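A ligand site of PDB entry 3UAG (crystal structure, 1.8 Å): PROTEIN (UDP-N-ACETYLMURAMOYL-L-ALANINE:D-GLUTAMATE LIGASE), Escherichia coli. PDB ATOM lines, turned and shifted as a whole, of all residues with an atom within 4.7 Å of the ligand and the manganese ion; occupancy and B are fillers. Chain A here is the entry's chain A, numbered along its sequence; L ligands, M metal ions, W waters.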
ATOM      1  N   ILE A  11      10.033  12.823  20.457  1.00  0.00           N
ATOM      2  CA  ILE A  11      10.295  14.143  21.032  1.00  0.00           C
ATOM      3  C   ILE A  11      10.119  15.211  19.966  1.00  0.00           C
ATOM      4  O   ILE A  11      10.765  15.155  18.912  1.00  0.00           O
ATOM      5  CB  ILE A  11      11.718  14.244  21.579  1.00  0.00           C
ATOM      6  CG1 ILE A  11      11.973  13.120  22.597  1.00  0.00           C
ATOM      7  CG2 ILE A  11      11.943  15.621  22.219  1.00  0.00           C
ATOM      8  CD1 ILE A  11      13.448  13.002  23.001  1.00  0.00           C
ATOM      9  N   GLY A  12       9.234  16.167  20.218  1.00  0.00           N
ATOM     10  CA  GLY A  12       9.017  17.264  19.308  1.00  0.00           C
ATOM     11  C   GLY A  12       7.595  17.225  18.802  1.00  0.00           C
ATOM     12  O   GLY A  12       7.178  16.216  18.245  1.00  0.00           O
ATOM     13  N   GLY A  14       6.386  19.552  16.573  1.00  0.00           N
ATOM     14  CA  GLY A  14       6.318  20.413  15.409  1.00  0.00           C
ATOM     15  C   GLY A  14       5.905  19.578  14.197  1.00  0.00           C
ATOM     16  O   GLY A  14       5.241  18.536  14.330  1.00  0.00           O
ATOM     17  N   LEU A  15       6.399  19.970  13.029  1.00  0.00           N
ATOM     18  CA  LEU A  15       6.052  19.286  11.780  1.00  0.00           C
ATOM     19  C   LEU A  15       6.599  17.873  11.814  1.00  0.00           C
ATOM     20  O   LEU A  15       5.904  16.936  11.424  1.00  0.00           O
ATOM     21  CB  LEU A  15       6.648  19.990  10.564  1.00  0.00           C
ATOM     22  CG  LEU A  15       6.283  21.433  10.295  1.00  0.00           C
ATOM     23  CD1 LEU A  15       7.046  21.924   9.068  1.00  0.00           C
ATOM     24  CD2 LEU A  15       4.797  21.537  10.091  1.00  0.00           C
ATOM     25  N   THR A  16       7.856  17.734  12.201  1.00  0.00           N
ATOM     26  CA  THR A  16       8.467  16.412  12.251  1.00  0.00           C
ATOM     27  C   THR A  16       7.732  15.459  13.188  1.00  0.00           C
ATOM     28  O   THR A  16       7.372  14.360  12.790  1.00  0.00           O
ATOM     29  CB  THR A  16       9.924  16.489  12.665  1.00  0.00           C
ATOM     30  OG1 THR A  16      10.628  17.338  11.743  1.00  0.00           O
ATOM     31  CG2 THR A  16      10.550  15.075  12.685  1.00  0.00           C
ATOM     32  N   GLY A  17       7.524  15.890  14.432  1.00  0.00           N
ATOM     33  CA  GLY A  17       6.865  15.040  15.400  1.00  0.00           C
ATOM     34  C   GLY A  17       5.492  14.607  14.927  1.00  0.00           C
ATOM     35  O   GLY A  17       5.113  13.440  15.124  1.00  0.00           O
ATOM     36  N   MET A  34       6.404  14.013  23.430  1.00  0.00           N
ATOM     37  CA  MET A  34       6.715  15.026  24.431  1.00  0.00           C
ATOM     38  C   MET A  34       7.428  16.178  23.754  1.00  0.00           C
ATOM     39  O   MET A  34       8.009  16.002  22.696  1.00  0.00           O
ATOM     40  CB  MET A  34       7.596  14.426  25.527  1.00  0.00           C
ATOM     41  CG  MET A  34       8.994  14.057  25.069  1.00  0.00           C
ATOM     42  SD  MET A  34      10.021  13.271  26.322  1.00  0.00           S
ATOM     43  CE  MET A  34       8.998  11.878  26.815  1.00  0.00           C
ATOM     44  N   ASP A  35       7.488  17.323  24.426  1.00  0.00           N
ATOM     45  CA  ASP A  35       8.177  18.497  23.895  1.00  0.00           C
ATOM     46  C   ASP A  35       8.523  19.369  25.103  1.00  0.00           C
ATOM     47  O   ASP A  35       7.747  19.442  26.049  1.00  0.00           O
ATOM     48  CB  ASP A  35       7.221  19.266  22.963  1.00  0.00           C
ATOM     49  CG  ASP A  35       7.944  20.261  22.058  1.00  0.00           C
ATOM     50  OD1 ASP A  35       8.570  21.206  22.562  1.00  0.00           O
ATOM     51  OD2 ASP A  35       7.843  20.109  20.837  1.00  0.00           O
ATOM     52  N   THR A  36       9.726  19.955  25.119  1.00  0.00           N
ATOM     53  CA  THR A  36      10.093  20.847  26.226  1.00  0.00           C
ATOM     54  C   THR A  36       9.276  22.153  26.243  1.00  0.00           C
ATOM     55  O   THR A  36       9.154  22.787  27.311  1.00  0.00           O
ATOM     56  CB  THR A  36      11.590  21.214  26.197  1.00  0.00           C
ATOM     57  OG1 THR A  36      11.861  22.017  25.055  1.00  0.00           O
ATOM     58  CG2 THR A  36      12.434  19.985  26.148  1.00  0.00           C
ATOM     59  N   ARG A  37       8.722  22.559  25.102  1.00  0.00           N
ATOM     60  CA  ARG A  37       7.831  23.729  25.051  1.00  0.00           C
ATOM     61  C   ARG A  37       6.499  23.432  25.733  1.00  0.00           C
ATOM     62  O   ARG A  37       5.957  22.334  25.636  1.00  0.00           O
ATOM     63  CB  ARG A  37       7.584  24.161  23.613  1.00  0.00           C
ATOM     64  CG  ARG A  37       8.845  24.661  22.904  1.00  0.00           C
ATOM     65  CD  ARG A  37       8.689  24.730  21.385  1.00  0.00           C
ATOM     66  NE  ARG A  37       8.535  23.414  20.772  1.00  0.00           N
ATOM     67  CZ  ARG A  37       8.380  23.209  19.473  1.00  0.00           C
ATOM     68  NH1 ARG A  37       8.354  24.243  18.633  1.00  0.00           N
ATOM     69  NH2 ARG A  37       8.399  21.985  18.972  1.00  0.00           N
ATOM     70  N   LEU A  57      11.074  17.374  29.109  1.00  0.00           N
ATOM     71  CA  LEU A  57      11.182  15.976  28.687  1.00  0.00           C
ATOM     72  C   LEU A  57      10.816  15.095  29.888  1.00  0.00           C
ATOM     73  O   LEU A  57      11.159  15.409  31.015  1.00  0.00           O
ATOM     74  CB  LEU A  57      12.593  15.658  28.196  1.00  0.00           C
ATOM     75  CG  LEU A  57      13.046  16.453  26.959  1.00  0.00           C
ATOM     76  CD1 LEU A  57      14.235  15.782  26.282  1.00  0.00           C
ATOM     77  CD2 LEU A  57      11.880  16.579  25.993  1.00  0.00           C
ATOM     78  N   SER A  71      13.018  14.650  17.161  1.00  0.00           N
ATOM     79  CA  SER A  71      12.943  15.696  16.121  1.00  0.00           C
ATOM     80  C   SER A  71      14.274  16.439  16.016  1.00  0.00           C
ATOM     81  O   SER A  71      15.038  16.512  16.985  1.00  0.00           O
ATOM     82  CB  SER A  71      11.837  16.689  16.438  1.00  0.00           C
ATOM     83  OG  SER A  71      10.559  16.084  16.307  1.00  0.00           O
ATOM     84  N   PRO A  72      14.561  17.042  14.856  1.00  0.00           N
ATOM     85  CA  PRO A  72      15.878  17.680  14.738  1.00  0.00           C
ATOM     86  C   PRO A  72      16.061  18.870  15.680  1.00  0.00           C
ATOM     87  O   PRO A  72      17.179  19.238  16.006  1.00  0.00           O
ATOM     88  CB  PRO A  72      15.947  18.090  13.254  1.00  0.00           C
ATOM     89  CG  PRO A  72      14.483  18.221  12.836  1.00  0.00           C
ATOM     90  CD  PRO A  72      13.775  17.104  13.616  1.00  0.00           C
ATOM     91  N   GLY A  73      14.950  19.446  16.142  1.00  0.00           N
ATOM     92  CA  GLY A  73      15.003  20.591  17.042  1.00  0.00           C
ATOM     93  C   GLY A  73      15.359  20.302  18.496  1.00  0.00           C
ATOM     94  O   GLY A  73      15.417  21.239  19.294  1.00  0.00           O
ATOM     95  N   ILE A  74      15.516  19.048  18.886  1.00  0.00           N
ATOM     96  CA  ILE A  74      16.010  18.737  20.226  1.00  0.00           C
ATOM     97  C   ILE A  74      17.447  18.231  20.117  1.00  0.00           C
ATOM     98  O   ILE A  74      17.750  17.396  19.266  1.00  0.00           O
ATOM     99  CB  ILE A  74      15.093  17.683  20.979  1.00  0.00           C
ATOM    100  CG1 ILE A  74      15.529  17.540  22.452  1.00  0.00           C
ATOM    101  CG2 ILE A  74      15.137  16.304  20.300  1.00  0.00           C
ATOM    102  CD1 ILE A  74      14.891  18.569  23.364  1.00  0.00           C
ATOM    103  N   ASP A  94      13.469  11.215  12.167  1.00  0.00           N
ATOM    104  CA  ASP A  94      12.515  10.870  11.137  1.00  0.00           C
ATOM    105  C   ASP A  94      13.230  10.479   9.850  1.00  0.00           C
ATOM    106  O   ASP A  94      12.741   9.619   9.112  1.00  0.00           O
ATOM    107  CB  ASP A  94      11.526  12.012  10.850  1.00  0.00           C
ATOM    108  CG  ASP A  94      12.181  13.240  10.213  1.00  0.00           C
ATOM    109  OD1 ASP A  94      13.202  13.711  10.763  1.00  0.00           O
ATOM    110  OD2 ASP A  94      11.596  13.814   9.266  1.00  0.00           O
ATOM    111  N   LYS A 115      21.203  24.355   0.188  1.00  0.00           N
ATOM    112  CA  LYS A 115      20.562  23.019   0.195  1.00  0.00           C
ATOM    113  C   LYS A 115      19.172  23.005  -0.526  1.00  0.00           C
ATOM    114  O   LYS A 115      18.915  22.124  -1.358  1.00  0.00           O
ATOM    115  CB  LYS A 115      20.388  22.455   1.619  1.00  0.00           C
ATOM    116  CG  LYS A 115      21.635  22.341   2.478  1.00  0.00           C
ATOM    117  CD  LYS A 115      21.291  21.728   3.884  1.00  0.00           C
ATOM    118  CE  LYS A 115      20.533  22.679   4.794  1.00  0.00           C
ATOM    119  NZ  LYS A 115      21.328  23.898   5.055  1.00  0.00           N
ATOM    120  N   GLY A 137      12.265  16.670   3.197  1.00  0.00           N
ATOM    121  CA  GLY A 137      13.293  16.778   4.230  1.00  0.00           C
ATOM    122  C   GLY A 137      13.254  18.160   4.852  1.00  0.00           C
ATOM    123  O   GLY A 137      12.178  18.783   5.001  1.00  0.00           O
ATOM    124  N   ASN A 138      14.428  18.687   5.150  1.00  0.00           N
ATOM    125  CA  ASN A 138      14.576  19.955   5.859  1.00  0.00           C
ATOM    126  C   ASN A 138      14.030  21.116   5.028  1.00  0.00           C
ATOM    127  O   ASN A 138      13.734  22.186   5.569  1.00  0.00           O
ATOM    128  CB  ASN A 138      16.051  20.171   6.190  1.00  0.00           C
ATOM    129  CG  ASN A 138      16.275  21.386   7.102  1.00  0.00           C
ATOM    130  OD1 ASN A 138      15.826  21.397   8.249  1.00  0.00           O
ATOM    131  ND2 ASN A 138      16.920  22.430   6.572  1.00  0.00           N
ATOM    132  N   ILE A 139      13.840  20.881   3.722  1.00  0.00           N
ATOM    133  CA  ILE A 139      13.219  21.869   2.841  1.00  0.00           C
ATOM    134  C   ILE A 139      11.812  22.254   3.300  1.00  0.00           C
ATOM    135  O   ILE A 139      11.323  23.318   2.940  1.00  0.00           O
ATOM    136  CB  ILE A 139      13.183  21.371   1.358  1.00  0.00           C
ATOM    137  CG1 ILE A 139      12.909  22.542   0.409  1.00  0.00           C
ATOM    138  CG2 ILE A 139      12.136  20.262   1.185  1.00  0.00           C
ATOM    139  CD1 ILE A 139      13.308  22.250  -1.019  1.00  0.00           C
ATOM    140  N   GLY A 140      11.132  21.352   4.009  1.00  0.00           N
ATOM    141  CA  GLY A 140       9.872  21.713   4.646  1.00  0.00           C
ATOM    142  C   GLY A 140       8.729  20.723   4.591  1.00  0.00           C
ATOM    143  O   GLY A 140       7.695  20.943   5.210  1.00  0.00           O
ATOM    144  N   PRO A 142       8.029  17.046   5.497  1.00  0.00           N
ATOM    145  CA  PRO A 142       8.631  15.967   6.287  1.00  0.00           C
ATOM    146  C   PRO A 142       8.816  14.724   5.449  1.00  0.00           C
ATOM    147  O   PRO A 142       7.869  14.287   4.788  1.00  0.00           O
ATOM    148  CB  PRO A 142       7.619  15.770   7.418  1.00  0.00           C
ATOM    149  CG  PRO A 142       7.126  17.157   7.647  1.00  0.00           C
ATOM    150  CD  PRO A 142       6.923  17.681   6.241  1.00  0.00           C
ATOM    151  N   SER A 159      19.489  18.483   7.106  1.00  0.00           N
ATOM    152  CA  SER A 159      20.249  19.377   7.985  1.00  0.00           C
ATOM    153  C   SER A 159      21.294  18.574   8.743  1.00  0.00           C
ATOM    154  O   SER A 159      21.167  17.350   8.897  1.00  0.00           O
ATOM    155  CB  SER A 159      19.303  20.038   8.980  1.00  0.00           C
ATOM    156  OG  SER A 159      18.785  19.068   9.875  1.00  0.00           O
ATOM    157  N   PHE A 161      21.422  18.588  11.888  1.00  0.00           N
ATOM    158  CA  PHE A 161      20.694  18.034  13.028  1.00  0.00           C
ATOM    159  C   PHE A 161      20.104  16.690  12.645  1.00  0.00           C
ATOM    160  O   PHE A 161      20.164  15.742  13.432  1.00  0.00           O
ATOM    161  CB  PHE A 161      19.544  18.925  13.441  1.00  0.00           C
ATOM    162  CG  PHE A 161      19.962  20.283  13.912  1.00  0.00           C
ATOM    163  CD1 PHE A 161      21.237  20.502  14.454  1.00  0.00           C
ATOM    164  CD2 PHE A 161      19.055  21.352  13.819  1.00  0.00           C
ATOM    165  CE1 PHE A 161      21.601  21.769  14.894  1.00  0.00           C
ATOM    166  CE2 PHE A 161      19.411  22.626  14.267  1.00  0.00           C
ATOM    167  CZ  PHE A 161      20.674  22.840  14.803  1.00  0.00           C
ATOM    168  N   GLN A 162      19.454  16.646  11.469  1.00  0.00           N
ATOM    169  CA  GLN A 162      18.878  15.383  10.935  1.00  0.00           C
ATOM    170  C   GLN A 162      19.934  14.274  10.740  1.00  0.00           C
ATOM    171  O   GLN A 162      19.716  13.124  11.116  1.00  0.00           O
ATOM    172  CB  GLN A 162      18.145  15.624   9.611  1.00  0.00           C
ATOM    173  CG  GLN A 162      16.810  16.356   9.771  1.00  0.00           C
ATOM    174  CD  GLN A 162      16.277  16.835   8.456  1.00  0.00           C
ATOM    175  OE1 GLN A 162      17.034  17.161   7.558  1.00  0.00           O
ATOM    176  NE2 GLN A 162      14.958  16.976   8.360  1.00  0.00           N
ATOM    177  N   ASP A 182      27.661  27.990  11.439  1.00  0.00           N
ATOM    178  CA  ASP A 182      26.225  28.098  11.622  1.00  0.00           C
ATOM    179  C   ASP A 182      25.908  27.164  12.765  1.00  0.00           C
ATOM    180  O   ASP A 182      26.745  26.323  13.105  1.00  0.00           O
ATOM    181  CB  ASP A 182      25.498  27.648  10.356  1.00  0.00           C
ATOM    182  CG  ASP A 182      24.026  28.090  10.299  1.00  0.00           C
ATOM    183  OD1 ASP A 182      23.509  28.723  11.260  1.00  0.00           O
ATOM    184  OD2 ASP A 182      23.404  27.841   9.239  1.00  0.00           O
ATOM    185  N   HIS A 183      24.761  27.369  13.393  1.00  0.00           N
ATOM    186  CA  HIS A 183      24.238  26.443  14.384  1.00  0.00           C
ATOM    187  C   HIS A 183      25.170  26.209  15.569  1.00  0.00           C
ATOM    188  O   HIS A 183      25.115  25.171  16.217  1.00  0.00           O
ATOM    189  CB  HIS A 183      23.914  25.108  13.714  1.00  0.00           C
ATOM    190  CG  HIS A 183      22.803  25.223  12.707  1.00  0.00           C
ATOM    191  ND1 HIS A 183      21.538  25.651  13.008  1.00  0.00           N
ATOM    192  CD2 HIS A 183      22.829  25.058  11.352  1.00  0.00           C
ATOM    193  CE1 HIS A 183      20.833  25.733  11.853  1.00  0.00           C
ATOM    194  NE2 HIS A 183      21.588  25.377  10.822  1.00  0.00           N
ATOM    195  N   KCX A 198      27.722  16.743   9.379  1.00  0.00           N
ATOM    196  CA  KCX A 198      27.487  16.759   7.934  1.00  0.00           C
ATOM    197  CB  KCX A 198      27.839  18.120   7.350  1.00  0.00           C
ATOM    198  CG  KCX A 198      26.929  19.223   7.787  1.00  0.00           C
ATOM    199  CD  KCX A 198      27.030  20.399   6.826  1.00  0.00           C
ATOM    200  CE  KCX A 198      26.170  21.573   7.285  1.00  0.00           C
ATOM    201  NZ  KCX A 198      24.733  21.253   7.249  1.00  0.00           N
ATOM    202  C   KCX A 198      28.221  15.643   7.171  1.00  0.00           C
ATOM    203  O   KCX A 198      27.665  15.054   6.255  1.00  0.00           O
ATOM    204  CX  KCX A 198      23.766  22.081   7.640  1.00  0.00           C
ATOM    205  OQ1 KCX A 198      24.034  23.225   8.072  1.00  0.00           O
ATOM    206  OQ2 KCX A 198      22.558  21.749   7.581  1.00  0.00           O
ATOM    207  N   LYS A 319      15.657  33.697   3.836  1.00  0.00           N
ATOM    208  CA  LYS A 319      16.319  32.414   4.055  1.00  0.00           C
ATOM    209  C   LYS A 319      17.838  32.560   4.199  1.00  0.00           C
ATOM    210  O   LYS A 319      18.550  31.543   4.300  1.00  0.00           O
ATOM    211  CB  LYS A 319      16.021  31.445   2.921  1.00  0.00           C
ATOM    212  CG  LYS A 319      15.453  30.146   3.402  1.00  0.00           C
ATOM    213  CD  LYS A 319      16.318  29.467   4.436  1.00  0.00           C
ATOM    214  CE  LYS A 319      15.734  28.112   4.821  1.00  0.00           C
ATOM    215  NZ  LYS A 319      16.801  27.164   5.258  1.00  0.00           N
ATOM    216  N   LEU A 416      13.157  32.315  14.617  1.00  0.00           N
ATOM    217  CA  LEU A 416      12.204  31.739  15.556  1.00  0.00           C
ATOM    218  C   LEU A 416      12.070  32.507  16.856  1.00  0.00           C
ATOM    219  O   LEU A 416      11.124  32.258  17.592  1.00  0.00           O
ATOM    220  CB  LEU A 416      12.517  30.266  15.849  1.00  0.00           C
ATOM    221  CG  LEU A 416      12.325  29.286  14.675  1.00  0.00           C
ATOM    222  CD1 LEU A 416      12.262  27.841  15.219  1.00  0.00           C
ATOM    223  CD2 LEU A 416      11.019  29.608  13.902  1.00  0.00           C
ATOM    224  N   PHE A 422      10.739  31.161   8.847  1.00  0.00           N
ATOM    225  CA  PHE A 422      11.367  32.172   7.988  1.00  0.00           C
ATOM    226  C   PHE A 422      10.415  32.611   6.871  1.00  0.00           C
ATOM    227  O   PHE A 422      10.518  33.746   6.384  1.00  0.00           O
ATOM    228  CB  PHE A 422      12.714  31.654   7.402  1.00  0.00           C
ATOM    229  CG  PHE A 422      12.564  30.606   6.319  1.00  0.00           C
ATOM    230  CD1 PHE A 422      12.309  30.966   4.982  1.00  0.00           C
ATOM    231  CD2 PHE A 422      12.659  29.229   6.640  1.00  0.00           C
ATOM    232  CE1 PHE A 422      12.127  30.009   3.988  1.00  0.00           C
ATOM    233  CE2 PHE A 422      12.473  28.243   5.643  1.00  0.00           C
ATOM    234  CZ  PHE A 422      12.213  28.632   4.324  1.00  0.00           C
HETATM  235  N1  LIG L   1      11.922  22.671  20.301  1.00  0.00           N
HETATM  236  C1  LIG L   1      12.013  22.777  21.683  1.00  0.00           C
HETATM  237  N2  LIG L   1      11.886  21.571  22.409  1.00  0.00           N
HETATM  238  C2  LIG L   1      11.513  20.312  21.871  1.00  0.00           C
HETATM  239  C3  LIG L   1      11.554  20.281  20.411  1.00  0.00           C
HETATM  240  C4  LIG L   1      11.738  21.436  19.704  1.00  0.00           C
HETATM  241  O1  LIG L   1      12.204  23.851  22.230  1.00  0.00           O
HETATM  242  O2  LIG L   1      11.161  19.363  22.581  1.00  0.00           O
HETATM  243  C5  LIG L   1      12.011  23.928  19.540  1.00  0.00           C
HETATM  244  C6  LIG L   1      13.240  23.672  18.780  1.00  0.00           C
HETATM  245  O3  LIG L   1      14.457  23.928  19.408  1.00  0.00           O
HETATM  246  C7  LIG L   1      13.200  24.157  17.426  1.00  0.00           C
HETATM  247  C8  LIG L   1      11.740  24.325  17.296  1.00  0.00           C
HETATM  248  O4  LIG L   1      11.107  23.833  18.511  1.00  0.00           O
HETATM  249  O5  LIG L   1      13.976  25.293  17.284  1.00  0.00           O
HETATM  250  C9  LIG L   1      11.381  23.433  16.081  1.00  0.00           C
HETATM  251  O6  LIG L   1      11.957  22.104  16.198  1.00  0.00           O
HETATM  252  P1  LIG L   1      11.240  20.853  15.549  1.00  0.00           P
HETATM  253  O7  LIG L   1      12.253  19.774  15.604  1.00  0.00           O
HETATM  254  O8  LIG L   1       9.942  20.656  16.151  1.00  0.00           O
HETATM  255  O9  LIG L   1      11.102  21.465  14.080  1.00  0.00           O
HETATM  256  P2  LIG L   1       9.962  21.046  13.004  1.00  0.00           P
HETATM  257  O10 LIG L   1       8.716  21.861  13.049  1.00  0.00           O
HETATM  258  O11 LIG L   1       9.741  19.627  12.944  1.00  0.00           O
HETATM  259  O12 LIG L   1      10.792  21.422  11.676  1.00  0.00           O
HETATM  260  C10 LIG L   1      11.961  20.661  11.400  1.00  0.00           C
HETATM  261  C11 LIG L   1      13.043  21.581  10.834  1.00  0.00           C
HETATM  262  N3  LIG L   1      13.410  22.558  11.842  1.00  0.00           N
HETATM  263  C12 LIG L   1      14.507  22.378  12.588  1.00  0.00           C
HETATM  264  O13 LIG L   1      15.288  21.446  12.377  1.00  0.00           O
HETATM  265  C13 LIG L   1      14.768  23.373  13.721  1.00  0.00           C
HETATM  266  C14 LIG L   1      12.444  22.229   9.574  1.00  0.00           C
HETATM  267  O14 LIG L   1      13.400  23.085   8.929  1.00  0.00           O
HETATM  268  C15 LIG L   1      12.096  21.142   8.577  1.00  0.00           C
HETATM  269  O15 LIG L   1      11.587  21.724   7.382  1.00  0.00           O
HETATM  270  C16 LIG L   1      11.083  20.167   9.189  1.00  0.00           C
HETATM  271  O16 LIG L   1      11.605  19.651  10.446  1.00  0.00           O
HETATM  272  C17 LIG L   1      10.861  18.966   8.278  1.00  0.00           C
HETATM  273  O17 LIG L   1      12.054  18.192   8.156  1.00  0.00           O
HETATM  274  C18 LIG L   1      13.576  24.513   9.136  1.00  0.00           C
HETATM  275  C19 LIG L   1      14.799  24.888   9.887  1.00  0.00           C
HETATM  276  O18 LIG L   1      14.923  26.005  10.330  1.00  0.00           O
HETATM  277  C20 LIG L   1      13.060  25.359   7.955  1.00  0.00           C
HETATM  278  N4  LIG L   1      15.767  23.974   9.903  1.00  0.00           N
HETATM  279  C21 LIG L   1      17.124  24.328  10.313  1.00  0.00           C
HETATM  280  C22 LIG L   1      17.918  25.056   9.223  1.00  0.00           C
HETATM  281  O19 LIG L   1      17.575  24.890   8.023  1.00  0.00           O
HETATM  282  O20 LIG L   1      18.949  25.705   9.566  1.00  0.00           O
HETATM  283  C23 LIG L   1      17.883  23.106  10.820  1.00  0.00           C
HETATM  284 MN    MN M   1      20.820  25.406   8.900  1.00  0.00          MN
HETATM  285  O   HOH W   1      16.231  19.766  10.430  1.00  0.00           O
HETATM  286  O   HOH W   2      15.991  28.471   9.642  1.00  0.00           O
HETATM  287  O   HOH W   3      13.321  27.417  11.867  1.00  0.00           O
HETATM  288  O   HOH W   4      20.829  23.219   8.800  1.00  0.00           O
HETATM  289  O   HOH W   5      16.827  24.287  16.321  1.00  0.00           O
HETATM  290  O   HOH W   6       7.814  23.503  15.046  1.00  0.00           O
HETATM  291  O   HOH W   7      18.550  28.215  11.132  1.00  0.00           O
HETATM  292  O   HOH W   8       9.246  26.124  15.484  1.00  0.00           O
HETATM  293  O   HOH W   9      12.175  26.470  23.230  1.00  0.00           O
HETATM  294  O   HOH W  10      19.756  25.454   6.928  1.00  0.00           O
HETATM  295  O   HOH W  11       9.300  23.822   7.669  1.00  0.00           O
HETATM  296  O   HOH W  12      22.617  25.259   7.826  1.00  0.00           O
HETATM  297  O   HOH W  13      11.992  15.530   7.211  1.00  0.00           O
HETATM  298  O   HOH W  14      11.742  24.923  12.629  1.00  0.00           O
HETATM  299  O   HOH W  15      10.242  26.885   7.654  1.00  0.00           O
HETATM  300  O   HOH W  16       8.933  24.036  11.489  1.00  0.00           O
HETATM  301  O   HOH W  17      20.949  27.600   8.953  1.00  0.00           O
HETATM  302  O   HOH W  18       8.711  18.072  15.854  1.00  0.00           O
HETATM  303  O   HOH W  19      17.935  28.065   7.628  1.00  0.00           O
HETATM  304  O   HOH W  20      12.825  16.455  10.380  1.00  0.00           O
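The backbone carbonyl oxygen of Gly 137 sits at hydrogen-bond distance from an oxygen (O17) of the ligand, 3.2 Å away. An oxygen (O7) of the ligand sits at hydrogen-bond distance from the backbone NH (N) of Gly 73. An oxygen (O3) of the ligand lies within hydrogen-bond range of the backbone carbonyl oxygen (O) of Gly 73 (2.9 Å). The side-chain amide nitrogen of Asn 138 is in hydrogen-bond range of an oxygen (O19) of the ligand (2.9 Å). NH2 of Arg 37 lies within salt-bridge range of O8 of the ligand. An oxygen (O11) of the ligand sits at hydrogen-bond distance from the side-chain hydroxyl (OG1) of Thr 16. O11 of the ligand lies within hydrogen-bond range of N of Thr 16 (2.8 Å). NZ of Lys 319 is in salt-bridge range of O19 of the ligand. The backbone carbonyl oxygen (O) of Asn 138 is in hydrogen-bond range of an oxygen (O15) of the ligand (2.8 Å). A nitrogen (N2) of the ligand lies within hydrogen-bond range of the side-chain hydroxyl (OG1) of Thr 36 (2.7 Å). The side-chain carboxylate (OD1) of Asp 35 lies close to a nitrogen (N2) of the ligand. An oxygen (O2) of the ligand sits at hydrogen-bond distance from the backbone NH (N) of Thr 36, at 3.0 Å. An oxygen (O17) of the ligand lies within hydrogen-bond range of the side-chain amide nitrogen of Gln 162 (3.2 Å). N of Leu 15 is in hydrogen-bond range of O10 of the ligand, 3.0 Å away. The backbone NH (N) of Gly 140 lies close to an oxygen (O15) of the ligand.
N of Ser 159 is in hydrogen-bond range of OE1 of Gln 162 (2.8 Å). OQ2 of KCX 198 is in salt-bridge range of the side-chain amino group (NZ) of Lys 115 (3.5 Å). OG of Ser 71 lies within hydrogen-bond range of O of Ile 11, 2.8 Å away. The side-chain carboxylate (OD2) of Asp 182 sits close to a ring nitrogen (NE2) of His 183. The side-chain carboxylate (OD2) of Asp 35 lies within salt-bridge range of the guanidinium group (NH2) of Arg 37 (2.7 Å). The backbone NH (N) of Phe 161 lies close to the side-chain hydroxyl (OG) of Ser 159, at 3.4 Å.
CG2 of Ile 11 touches O2 of the ligand (3.8 Å). Gly 14 touches the ligand (CA to O10, 3.7 Å). Ser 71 touches the ligand (CB to O7, 3.2 Å). Pro 72 touches the ligand. CD1 of Ile 74 touches O2 of the ligand, 3.9 Å away. Ser 159 touches the ligand (CB to C23, 3.8 Å). Phe 161 touches the ligand. Leu 416 touches the ligand (CD1 to O5, 3.7 Å). CE2 of Phe 422 touches C20 of the ligand, at 3.7 Å. Hydrophobic or aromatic side chains within 4 Å of the ligand: Ile 11, Leu 15, Pro 72, Ile 74, Phe 161, His 183, Leu 416 and Phe 422. 21 residues have an atom within 4 Å of the ligand: Ile 11, Gly 14, Leu 15, Thr 16, Asp 35, Thr 36, Arg 37, Ser 71, Pro 72, Gly 73, Ile 74, Gly 137, Asn 138, Gly 140, Ser 159, Phe 161, Gln 162, His 183, Lys 319, Leu 416 and Phe 422. Along chain A the residues within 4 Å of the ligand span positions 11 to 422.
Asp 182 touches the manganese ion. OQ1 of KCX 198 touches the manganese ion, at 3.97 Å. Within 4 Å of the manganese ion: Asp 182, His 183 and KCX 198.
The manganese ion is bound by an oxygen (O20) of the ligand (2.0 Å), a ring nitrogen (NE2) of His 183 (2.1 Å), water W12 (2.1 Å), water W4 (2.2 Å), water W17 (2.2 Å) and water W10 (2.2 Å).
Water W12 lies within hydrogen-bond range of OQ1 of KCX 198, OD2 of Asp 182 and NZ of Lys 115. Water W1 lies within hydrogen-bond range of OG of Ser 159, O13 of the ligand and OD1 of Asn 138. Water W13 lies within hydrogen-bond range of OD2 of Asp 94, O17 of the ligand and NE2 of Gln 162. Water W18 lies within hydrogen-bond range of the side-chain hydroxyl (OG) of Ser 71 (2.8 Å), the backbone NH (N) of Gly 14 (2.8 Å), the backbone NH (N) of Gly 17 (2.9 Å), an oxygen (O8) of the ligand (2.9 Å) and the backbone carbonyl oxygen (O) of Gly 12 (3.4 Å). Water W20 lies within hydrogen-bond range of the side-chain hydroxyl (OG1) of Thr 16 (2.7 Å), the side-chain carboxylate (OD1) of Asp 94 (2.8 Å), an oxygen (O17) of the ligand (2.9 Å) and the side-chain amide nitrogen (NE2) of Gln 162 (3.0 Å). Water W19 lies within hydrogen-bond range of the side-chain amino group (NZ) of Lys 319 and an oxygen (O19) of the ligand.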
